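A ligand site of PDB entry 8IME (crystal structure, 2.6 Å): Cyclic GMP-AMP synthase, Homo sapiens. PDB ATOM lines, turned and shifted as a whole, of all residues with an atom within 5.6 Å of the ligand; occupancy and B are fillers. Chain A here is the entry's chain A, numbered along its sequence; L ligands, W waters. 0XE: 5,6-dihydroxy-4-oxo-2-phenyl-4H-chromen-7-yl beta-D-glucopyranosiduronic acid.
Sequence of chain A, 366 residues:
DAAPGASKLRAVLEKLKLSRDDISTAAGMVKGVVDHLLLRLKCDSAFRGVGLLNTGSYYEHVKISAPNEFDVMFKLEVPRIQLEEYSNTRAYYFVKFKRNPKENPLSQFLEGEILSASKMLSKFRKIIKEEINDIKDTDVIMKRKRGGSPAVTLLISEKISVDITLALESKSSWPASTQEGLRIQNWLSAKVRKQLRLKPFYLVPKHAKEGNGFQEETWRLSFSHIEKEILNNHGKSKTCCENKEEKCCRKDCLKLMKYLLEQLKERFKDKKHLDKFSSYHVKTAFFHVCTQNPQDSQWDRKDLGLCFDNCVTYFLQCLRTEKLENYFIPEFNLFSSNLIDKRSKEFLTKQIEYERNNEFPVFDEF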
ATOM      1  N   VAL A  62       8.956  22.018  23.237  1.00  0.00           N
ATOM      2  CA  VAL A  62       9.711  22.435  24.412  1.00  0.00           C
ATOM      3  C   VAL A  62       8.854  23.307  25.324  1.00  0.00           C
ATOM      4  O   VAL A  62       9.022  23.285  26.550  1.00  0.00           O
ATOM      5  CB  VAL A  62      11.004  23.159  23.984  1.00  0.00           C
ATOM      6  N   ASP A  71       9.836  22.632  17.789  1.00  0.00           N
ATOM      7  CA  ASP A  71      11.294  22.627  17.783  1.00  0.00           C
ATOM      8  C   ASP A  71      11.780  21.349  17.110  1.00  0.00           C
ATOM      9  O   ASP A  71      11.519  20.249  17.600  1.00  0.00           O
ATOM     10  CB  ASP A  71      11.864  22.735  19.198  1.00  0.00           C
ATOM     11  N   MET A  73      15.312  19.442  15.181  1.00  0.00           N
ATOM     12  CA  MET A  73      16.768  19.435  15.219  1.00  0.00           C
ATOM     13  C   MET A  73      17.296  18.746  13.971  1.00  0.00           C
ATOM     14  O   MET A  73      16.933  17.598  13.690  1.00  0.00           O
ATOM     15  CB  MET A  73      17.286  18.731  16.481  1.00  0.00           C
ATOM     16  CG  MET A  73      18.772  18.939  16.741  1.00  0.00           C
ATOM     17  SD  MET A  73      19.359  18.107  18.228  1.00  0.00           S
ATOM     18  CE  MET A  73      18.972  19.329  19.479  1.00  0.00           C
ATOM     19  N   TYR A  92      31.070  23.157  27.411  1.00  0.00           N
ATOM     20  CA  TYR A  92      31.357  23.899  26.194  1.00  0.00           C
ATOM     21  C   TYR A  92      32.694  23.453  25.631  1.00  0.00           C
ATOM     22  O   TYR A  92      33.648  23.254  26.390  1.00  0.00           O
ATOM     23  CB  TYR A  92      31.339  25.404  26.458  1.00  0.00           C
ATOM     24  CG  TYR A  92      29.972  25.915  26.836  1.00  0.00           C
ATOM     25  CD1 TYR A  92      29.518  25.839  28.143  1.00  0.00           C
ATOM     26  CD2 TYR A  92      29.114  26.448  25.878  1.00  0.00           C
ATOM     27  CE1 TYR A  92      28.255  26.289  28.492  1.00  0.00           C
ATOM     28  CE2 TYR A  92      27.853  26.909  26.219  1.00  0.00           C
ATOM     29  CZ  TYR A  92      27.434  26.822  27.530  1.00  0.00           C
ATOM     30  OH  TYR A  92      26.175  27.273  27.871  1.00  0.00           O
ATOM     31  N   VAL A 204      25.868  21.551  20.009  1.00  0.00           N
ATOM     32  CA  VAL A 204      25.009  22.620  19.507  1.00  0.00           C
ATOM     33  C   VAL A 204      25.744  23.951  19.630  1.00  0.00           C
ATOM     34  O   VAL A 204      26.616  24.096  20.499  1.00  0.00           O
ATOM     35  CB  VAL A 204      23.666  22.647  20.253  1.00  0.00           C
ATOM     36  CG1 VAL A 204      22.719  21.593  19.690  1.00  0.00           C
ATOM     37  CG2 VAL A 204      23.891  22.428  21.741  1.00  0.00           C
ATOM     38  N   ARG A 220      28.154  23.362  22.657  1.00  0.00           N
ATOM     39  CA  ARG A 220      27.698  22.807  23.919  1.00  0.00           C
ATOM     40  C   ARG A 220      27.221  21.370  23.723  1.00  0.00           C
ATOM     41  O   ARG A 220      26.600  21.046  22.705  1.00  0.00           O
ATOM     42  CB  ARG A 220      26.574  23.649  24.526  1.00  0.00           C
ATOM     43  CG  ARG A 220      25.966  23.059  25.782  1.00  0.00           C
ATOM     44  CD  ARG A 220      25.117  24.067  26.554  1.00  0.00           C
ATOM     45  NE  ARG A 220      23.981  24.609  25.810  1.00  0.00           N
ATOM     46  CZ  ARG A 220      23.008  23.891  25.259  1.00  0.00           C
ATOM     47  NH1 ARG A 220      22.974  22.569  25.351  1.00  0.00           N
ATOM     48  NH2 ARG A 220      22.034  24.517  24.605  1.00  0.00           N
ATOM     49  N   LEU A 221      27.516  20.512  24.700  1.00  0.00           N
ATOM     50  CA  LEU A 221      27.057  19.135  24.652  1.00  0.00           C
ATOM     51  C   LEU A 221      25.532  19.073  24.724  1.00  0.00           C
ATOM     52  O   LEU A 221      24.896  19.822  25.471  1.00  0.00           O
ATOM     53  CB  LEU A 221      27.661  18.327  25.811  1.00  0.00           C
ATOM     54  CG  LEU A 221      29.112  17.858  25.680  1.00  0.00           C
ATOM     55  CD1 LEU A 221      29.495  17.003  26.874  1.00  0.00           C
ATOM     56  CD2 LEU A 221      29.315  17.096  24.375  1.00  0.00           C
ATOM     57  N   SER A 222      24.953  18.162  23.947  1.00  0.00           N
ATOM     58  CA  SER A 222      23.512  17.977  23.887  1.00  0.00           C
ATOM     59  C   SER A 222      23.178  16.509  24.055  1.00  0.00           C
ATOM     60  O   SER A 222      23.722  15.658  23.331  1.00  0.00           O
ATOM     61  CB  SER A 222      22.927  18.507  22.576  1.00  0.00           C
ATOM     62  OG  SER A 222      21.533  18.692  22.676  1.00  0.00           O
ATOM     63  N   SER A 224      19.678  15.670  24.491  1.00  0.00           N
ATOM     64  CA  SER A 224      18.216  15.706  24.467  1.00  0.00           C
ATOM     65  C   SER A 224      17.626  14.400  23.955  1.00  0.00           C
ATOM     66  O   SER A 224      16.530  14.018  24.374  1.00  0.00           O
ATOM     67  CB  SER A 224      17.739  16.880  23.601  1.00  0.00           C
ATOM     68  OG  SER A 224      17.501  18.027  24.397  1.00  0.00           O
ATOM     69  N   GLU A 227      17.320  12.180  26.760  1.00  0.00           N
ATOM     70  CA  GLU A 227      16.240  12.643  27.630  1.00  0.00           C
ATOM     71  C   GLU A 227      14.885  12.154  27.126  1.00  0.00           C
ATOM     72  O   GLU A 227      14.048  11.681  27.900  1.00  0.00           O
ATOM     73  CB  GLU A 227      16.266  14.171  27.727  1.00  0.00           C
ATOM     74  CG  GLU A 227      17.384  14.714  28.601  1.00  0.00           C
ATOM     75  CD  GLU A 227      17.686  16.179  28.323  1.00  0.00           C
ATOM     76  OE1 GLU A 227      16.882  16.837  27.626  1.00  0.00           O
ATOM     77  OE2 GLU A 227      18.722  16.679  28.802  1.00  0.00           O
ATOM     78  N   ASP A 275      13.708  35.644  33.313  1.00  0.00           N
ATOM     79  CA  ASP A 275      14.189  35.481  31.946  1.00  0.00           C
ATOM     80  C   ASP A 275      15.238  34.378  31.840  1.00  0.00           C
ATOM     81  O   ASP A 275      15.309  33.686  30.814  1.00  0.00           O
ATOM     82  CB  ASP A 275      14.767  36.792  31.423  1.00  0.00           C
ATOM     83  CG  ASP A 275      13.693  37.771  31.009  1.00  0.00           C
ATOM     84  OD1 ASP A 275      12.494  37.409  31.082  1.00  0.00           O
ATOM     85  OD2 ASP A 275      14.031  38.899  30.598  1.00  0.00           O
ATOM     86  N   LYS A 276      16.040  34.180  32.886  1.00  0.00           N
ATOM     87  CA  LYS A 276      17.098  33.189  32.877  1.00  0.00           C
ATOM     88  C   LYS A 276      16.640  31.813  33.345  1.00  0.00           C
ATOM     89  O   LYS A 276      17.473  30.957  33.627  1.00  0.00           O
ATOM     90  CB  LYS A 276      18.271  33.677  33.722  1.00  0.00           C
ATOM     91  CG  LYS A 276      19.029  34.838  33.099  1.00  0.00           C
ATOM     92  CD  LYS A 276      20.085  35.390  34.035  1.00  0.00           C
ATOM     93  CE  LYS A 276      20.990  36.382  33.315  1.00  0.00           C
ATOM     94  NZ  LYS A 276      22.198  36.725  34.124  1.00  0.00           N
ATOM     95  N   PHE A 277      15.331  31.584  33.447  1.00  0.00           N
ATOM     96  CA  PHE A 277      14.790  30.292  33.833  1.00  0.00           C
ATOM     97  C   PHE A 277      14.109  29.647  32.636  1.00  0.00           C
ATOM     98  O   PHE A 277      13.499  30.329  31.814  1.00  0.00           O
ATOM     99  CB  PHE A 277      13.806  30.421  35.002  1.00  0.00           C
ATOM    100  CG  PHE A 277      14.448  30.872  36.275  1.00  0.00           C
ATOM    101  CD1 PHE A 277      15.257  30.005  36.999  1.00  0.00           C
ATOM    102  CD2 PHE A 277      14.236  32.150  36.758  1.00  0.00           C
ATOM    103  CE1 PHE A 277      15.845  30.414  38.179  1.00  0.00           C
ATOM    104  CE2 PHE A 277      14.830  32.561  37.929  1.00  0.00           C
ATOM    105  CZ  PHE A 277      15.634  31.693  38.639  1.00  0.00           C
ATOM    106  N   SER A 278      14.238  28.322  32.547  1.00  0.00           N
ATOM    107  CA  SER A 278      13.824  27.590  31.355  1.00  0.00           C
ATOM    108  C   SER A 278      13.175  26.284  31.773  1.00  0.00           C
ATOM    109  O   SER A 278      13.308  25.838  32.926  1.00  0.00           O
ATOM    110  CB  SER A 278      15.014  27.329  30.447  1.00  0.00           C
ATOM    111  OG  SER A 278      14.847  26.095  29.779  1.00  0.00           O
ATOM    112  N   SER A 279      12.471  25.660  30.832  1.00  0.00           N
ATOM    113  CA  SER A 279      11.952  24.330  31.096  1.00  0.00           C
ATOM    114  C   SER A 279      13.065  23.297  31.197  1.00  0.00           C
ATOM    115  O   SER A 279      12.800  22.159  31.609  1.00  0.00           O
ATOM    116  CB  SER A 279      10.932  23.943  30.019  1.00  0.00           C
ATOM    117  OG  SER A 279      11.569  23.757  28.762  1.00  0.00           O
ATOM    118  N   TYR A 280      14.293  23.662  30.843  1.00  0.00           N
ATOM    119  CA  TYR A 280      15.404  22.712  30.950  1.00  0.00           C
ATOM    120  C   TYR A 280      15.802  22.495  32.402  1.00  0.00           C
ATOM    121  O   TYR A 280      16.137  21.369  32.793  1.00  0.00           O
ATOM    122  CB  TYR A 280      16.602  23.201  30.137  1.00  0.00           C
ATOM    123  CG  TYR A 280      17.696  22.162  30.067  1.00  0.00           C
ATOM    124  CD1 TYR A 280      17.563  21.042  29.246  1.00  0.00           C
ATOM    125  CD2 TYR A 280      18.846  22.281  30.833  1.00  0.00           C
ATOM    126  CE1 TYR A 280      18.561  20.089  29.180  1.00  0.00           C
ATOM    127  CE2 TYR A 280      19.844  21.329  30.767  1.00  0.00           C
ATOM    128  CZ  TYR A 280      19.694  20.235  29.943  1.00  0.00           C
ATOM    129  OH  TYR A 280      20.684  19.280  29.872  1.00  0.00           O
ATOM    130  N   HIS A 281      15.800  23.554  33.221  1.00  0.00           N
ATOM    131  CA  HIS A 281      16.051  23.378  34.641  1.00  0.00           C
ATOM    132  C   HIS A 281      14.951  22.552  35.295  1.00  0.00           C
ATOM    133  O   HIS A 281      15.224  21.695  36.146  1.00  0.00           O
ATOM    134  CB  HIS A 281      16.188  24.725  35.351  1.00  0.00           C
ATOM    135  CG  HIS A 281      16.856  25.787  34.536  1.00  0.00           C
ATOM    136  ND1 HIS A 281      16.180  26.899  34.069  1.00  0.00           N
ATOM    137  CD2 HIS A 281      18.141  25.922  34.127  1.00  0.00           C
ATOM    138  CE1 HIS A 281      17.024  27.660  33.395  1.00  0.00           C
ATOM    139  NE2 HIS A 281      18.213  27.093  33.417  1.00  0.00           N
ATOM    140  N   LYS A 283      13.113  20.304  33.803  1.00  0.00           N
ATOM    141  CA  LYS A 283      13.343  18.924  33.377  1.00  0.00           C
ATOM    142  C   LYS A 283      14.581  18.335  34.027  1.00  0.00           C
ATOM    143  O   LYS A 283      14.638  17.127  34.258  1.00  0.00           O
ATOM    144  CB  LYS A 283      13.454  18.880  31.857  1.00  0.00           C
ATOM    145  CG  LYS A 283      13.316  17.495  31.252  1.00  0.00           C
ATOM    146  CD  LYS A 283      13.350  17.552  29.736  1.00  0.00           C
ATOM    147  CE  LYS A 283      14.531  18.382  29.250  1.00  0.00           C
ATOM    148  NZ  LYS A 283      14.620  18.391  27.764  1.00  0.00           N
ATOM    149  N   ASN A 326      23.783  19.723  35.911  1.00  0.00           N
ATOM    150  CA  ASN A 326      23.381  19.102  34.668  1.00  0.00           C
ATOM    151  C   ASN A 326      23.336  17.583  34.849  1.00  0.00           C
ATOM    152  O   ASN A 326      24.262  16.990  35.406  1.00  0.00           O
ATOM    153  CB  ASN A 326      24.356  19.489  33.546  1.00  0.00           C
ATOM    154  CG  ASN A 326      24.004  18.867  32.215  1.00  0.00           C
ATOM    155  OD1 ASN A 326      24.203  17.675  31.984  1.00  0.00           O
ATOM    156  ND2 ASN A 326      23.477  19.694  31.306  1.00  0.00           N
ATOM    157  N   PHE A 332      28.694  20.741  35.839  1.00  0.00           N
ATOM    158  CA  PHE A 332      28.077  21.911  35.220  1.00  0.00           C
ATOM    159  C   PHE A 332      26.873  22.307  36.069  1.00  0.00           C
ATOM    160  O   PHE A 332      25.843  21.624  36.058  1.00  0.00           O
ATOM    161  CB  PHE A 332      27.682  21.574  33.790  1.00  0.00           C
ATOM    162  CG  PHE A 332      26.987  22.696  33.040  1.00  0.00           C
ATOM    163  CD1 PHE A 332      27.111  24.016  33.453  1.00  0.00           C
ATOM    164  CD2 PHE A 332      26.224  22.409  31.923  1.00  0.00           C
ATOM    165  CE1 PHE A 332      26.465  25.024  32.751  1.00  0.00           C
ATOM    166  CE2 PHE A 332      25.578  23.418  31.221  1.00  0.00           C
ATOM    167  CZ  PHE A 332      25.701  24.726  31.641  1.00  0.00           C
ATOM    168  N   LEU A 334      23.849  24.488  36.796  1.00  0.00           N
ATOM    169  CA  LEU A 334      22.951  25.352  36.024  1.00  0.00           C
ATOM    170  C   LEU A 334      22.500  26.571  36.829  1.00  0.00           C
ATOM    171  O   LEU A 334      22.124  27.581  36.232  1.00  0.00           O
ATOM    172  CB  LEU A 334      21.745  24.540  35.552  1.00  0.00           C
ATOM    173  CG  LEU A 334      22.086  23.323  34.691  1.00  0.00           C
ATOM    174  CD1 LEU A 334      20.890  22.401  34.543  1.00  0.00           C
ATOM    175  CD2 LEU A 334      22.611  23.768  33.338  1.00  0.00           C
HETATM  176  C1  0XE L   1      16.636  29.493  28.342  1.00  0.00           C
HETATM  177  C2  0XE L   1      16.788  30.375  29.385  1.00  0.00           C
HETATM  178  C3  0XE L   1      17.742  30.133  30.351  1.00  0.00           C
HETATM  179  C4  0XE L   1      18.546  29.019  30.266  1.00  0.00           C
HETATM  180  C5  0XE L   1      18.408  28.109  29.212  1.00  0.00           C
HETATM  181  C6  0XE L   1      17.448  28.371  28.247  1.00  0.00           C
HETATM  182  C7  0XE L   1      19.297  26.926  29.132  1.00  0.00           C
HETATM  183  C8  0XE L   1      20.423  26.802  29.846  1.00  0.00           C
HETATM  184  C9  0XE L   1      21.279  25.641  29.754  1.00  0.00           C
HETATM  185  O9  0XE L   1      22.330  25.539  30.422  1.00  0.00           O
HETATM  186  O12 0XE L   1      18.884  25.955  28.279  1.00  0.00           O
HETATM  187  C11 0XE L   1      19.635  24.807  28.136  1.00  0.00           C
HETATM  188  C10 0XE L   1      20.818  24.617  28.842  1.00  0.00           C
HETATM  189  C17 0XE L   1      21.525  23.409  28.618  1.00  0.00           C
HETATM  190  O17 0XE L   1      22.681  23.161  29.274  1.00  0.00           O
HETATM  191  C16 0XE L   1      21.041  22.460  27.732  1.00  0.00           C
HETATM  192  O16 0XE L   1      21.739  21.310  27.538  1.00  0.00           O
HETATM  193  C14 0XE L   1      19.141  23.877  27.238  1.00  0.00           C
HETATM  194  C15 0XE L   1      19.848  22.698  27.042  1.00  0.00           C
HETATM  195  O18 0XE L   1      19.402  21.729  26.161  1.00  0.00           O
HETATM  196  C18 0XE L   1      18.298  22.065  25.332  1.00  0.00           C
HETATM  197  O22 0XE L   1      17.092  21.966  26.063  1.00  0.00           O
HETATM  198  C22 0XE L   1      15.963  22.436  25.319  1.00  0.00           C
HETATM  199  C23 0XE L   1      14.727  22.258  26.179  1.00  0.00           C
HETATM  200  O24 0XE L   1      13.889  23.145  26.222  1.00  0.00           O
HETATM  201  O23 0XE L   1      14.590  21.238  26.830  1.00  0.00           O
HETATM  202  C19 0XE L   1      18.241  21.104  24.160  1.00  0.00           C
HETATM  203  O19 0XE L   1      19.483  21.076  23.466  1.00  0.00           O
HETATM  204  C20 0XE L   1      17.123  21.576  23.250  1.00  0.00           C
HETATM  205  O20 0XE L   1      16.986  20.702  22.136  1.00  0.00           O
HETATM  206  C21 0XE L   1      15.801  21.692  24.002  1.00  0.00           C
HETATM  207  O21 0XE L   1      14.856  22.389  23.182  1.00  0.00           O
HETATM  208  O   HOH W   1      20.715  18.953  26.534  1.00  0.00           O
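NH1 of Arg 220 lies within hydrogen-bond range of O16 of the ligand (2.8 Å). NZ of Lys 283 lies within salt-bridge range of O23 of the ligand, at 3.0 Å. An oxygen (O19) of the ligand sits at hydrogen-bond distance from the side-chain hydroxyl of Ser 222 (3.2 Å). The side-chain hydroxyl of Tyr 280 lies within hydrogen-bond range of an oxygen (O16) of the ligand, at 3.3 Å. An oxygen (O24) of the ligand lies within hydrogen-bond range of the side-chain hydroxyl (OG) of Ser 279.
The backbone carbonyl oxygen (O) of Val 204 sits at hydrogen-bond distance from the backbone NH (N) of Arg 220 (2.7 Å). NZ of Lys 283 lies within salt-bridge range of OE1 of Glu 227 (2.7 Å). The side-chain hydroxyl (OG) of Ser 224 is in hydrogen-bond range of the side-chain carboxylate (OE1) of Glu 227, at 3.5 Å. The side-chain amide nitrogen (ND2) of Asn 326 is in hydrogen-bond range of the side-chain hydroxyl (OH) of Tyr 280 (3.2 Å). The side-chain carboxylate (OE2) of Glu 227 lies within hydrogen-bond range of the side-chain hydroxyl (OH) of Tyr 280. A ring nitrogen (ND1) of His 281 is in hydrogen-bond range of the backbone NH of Ser 278. The side-chain hydroxyl of Ser 279 lies within hydrogen-bond range of the backbone carbonyl oxygen of Val 62. N of Asn 326 is in hydrogen-bond range of O of Phe 332.
Residues that only touch the ligand: Ser 224 (3.2 Å), Lys 276 (3.4 Å), Leu 334 (3.4 Å), Ser 278 (3.4 Å), Phe 332 (3.5 Å), Met 73 (3.6 Å), Val 62 (3.7 Å), His 281 (3.7 Å) and Asp 275 (3.9 Å). Of the 21 residues printed, 14 come within 4 Å of the ligand.
Water W1 bridges O16 of the ligand (2.8 Å) and OH of Tyr 280 (3.4 Å).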
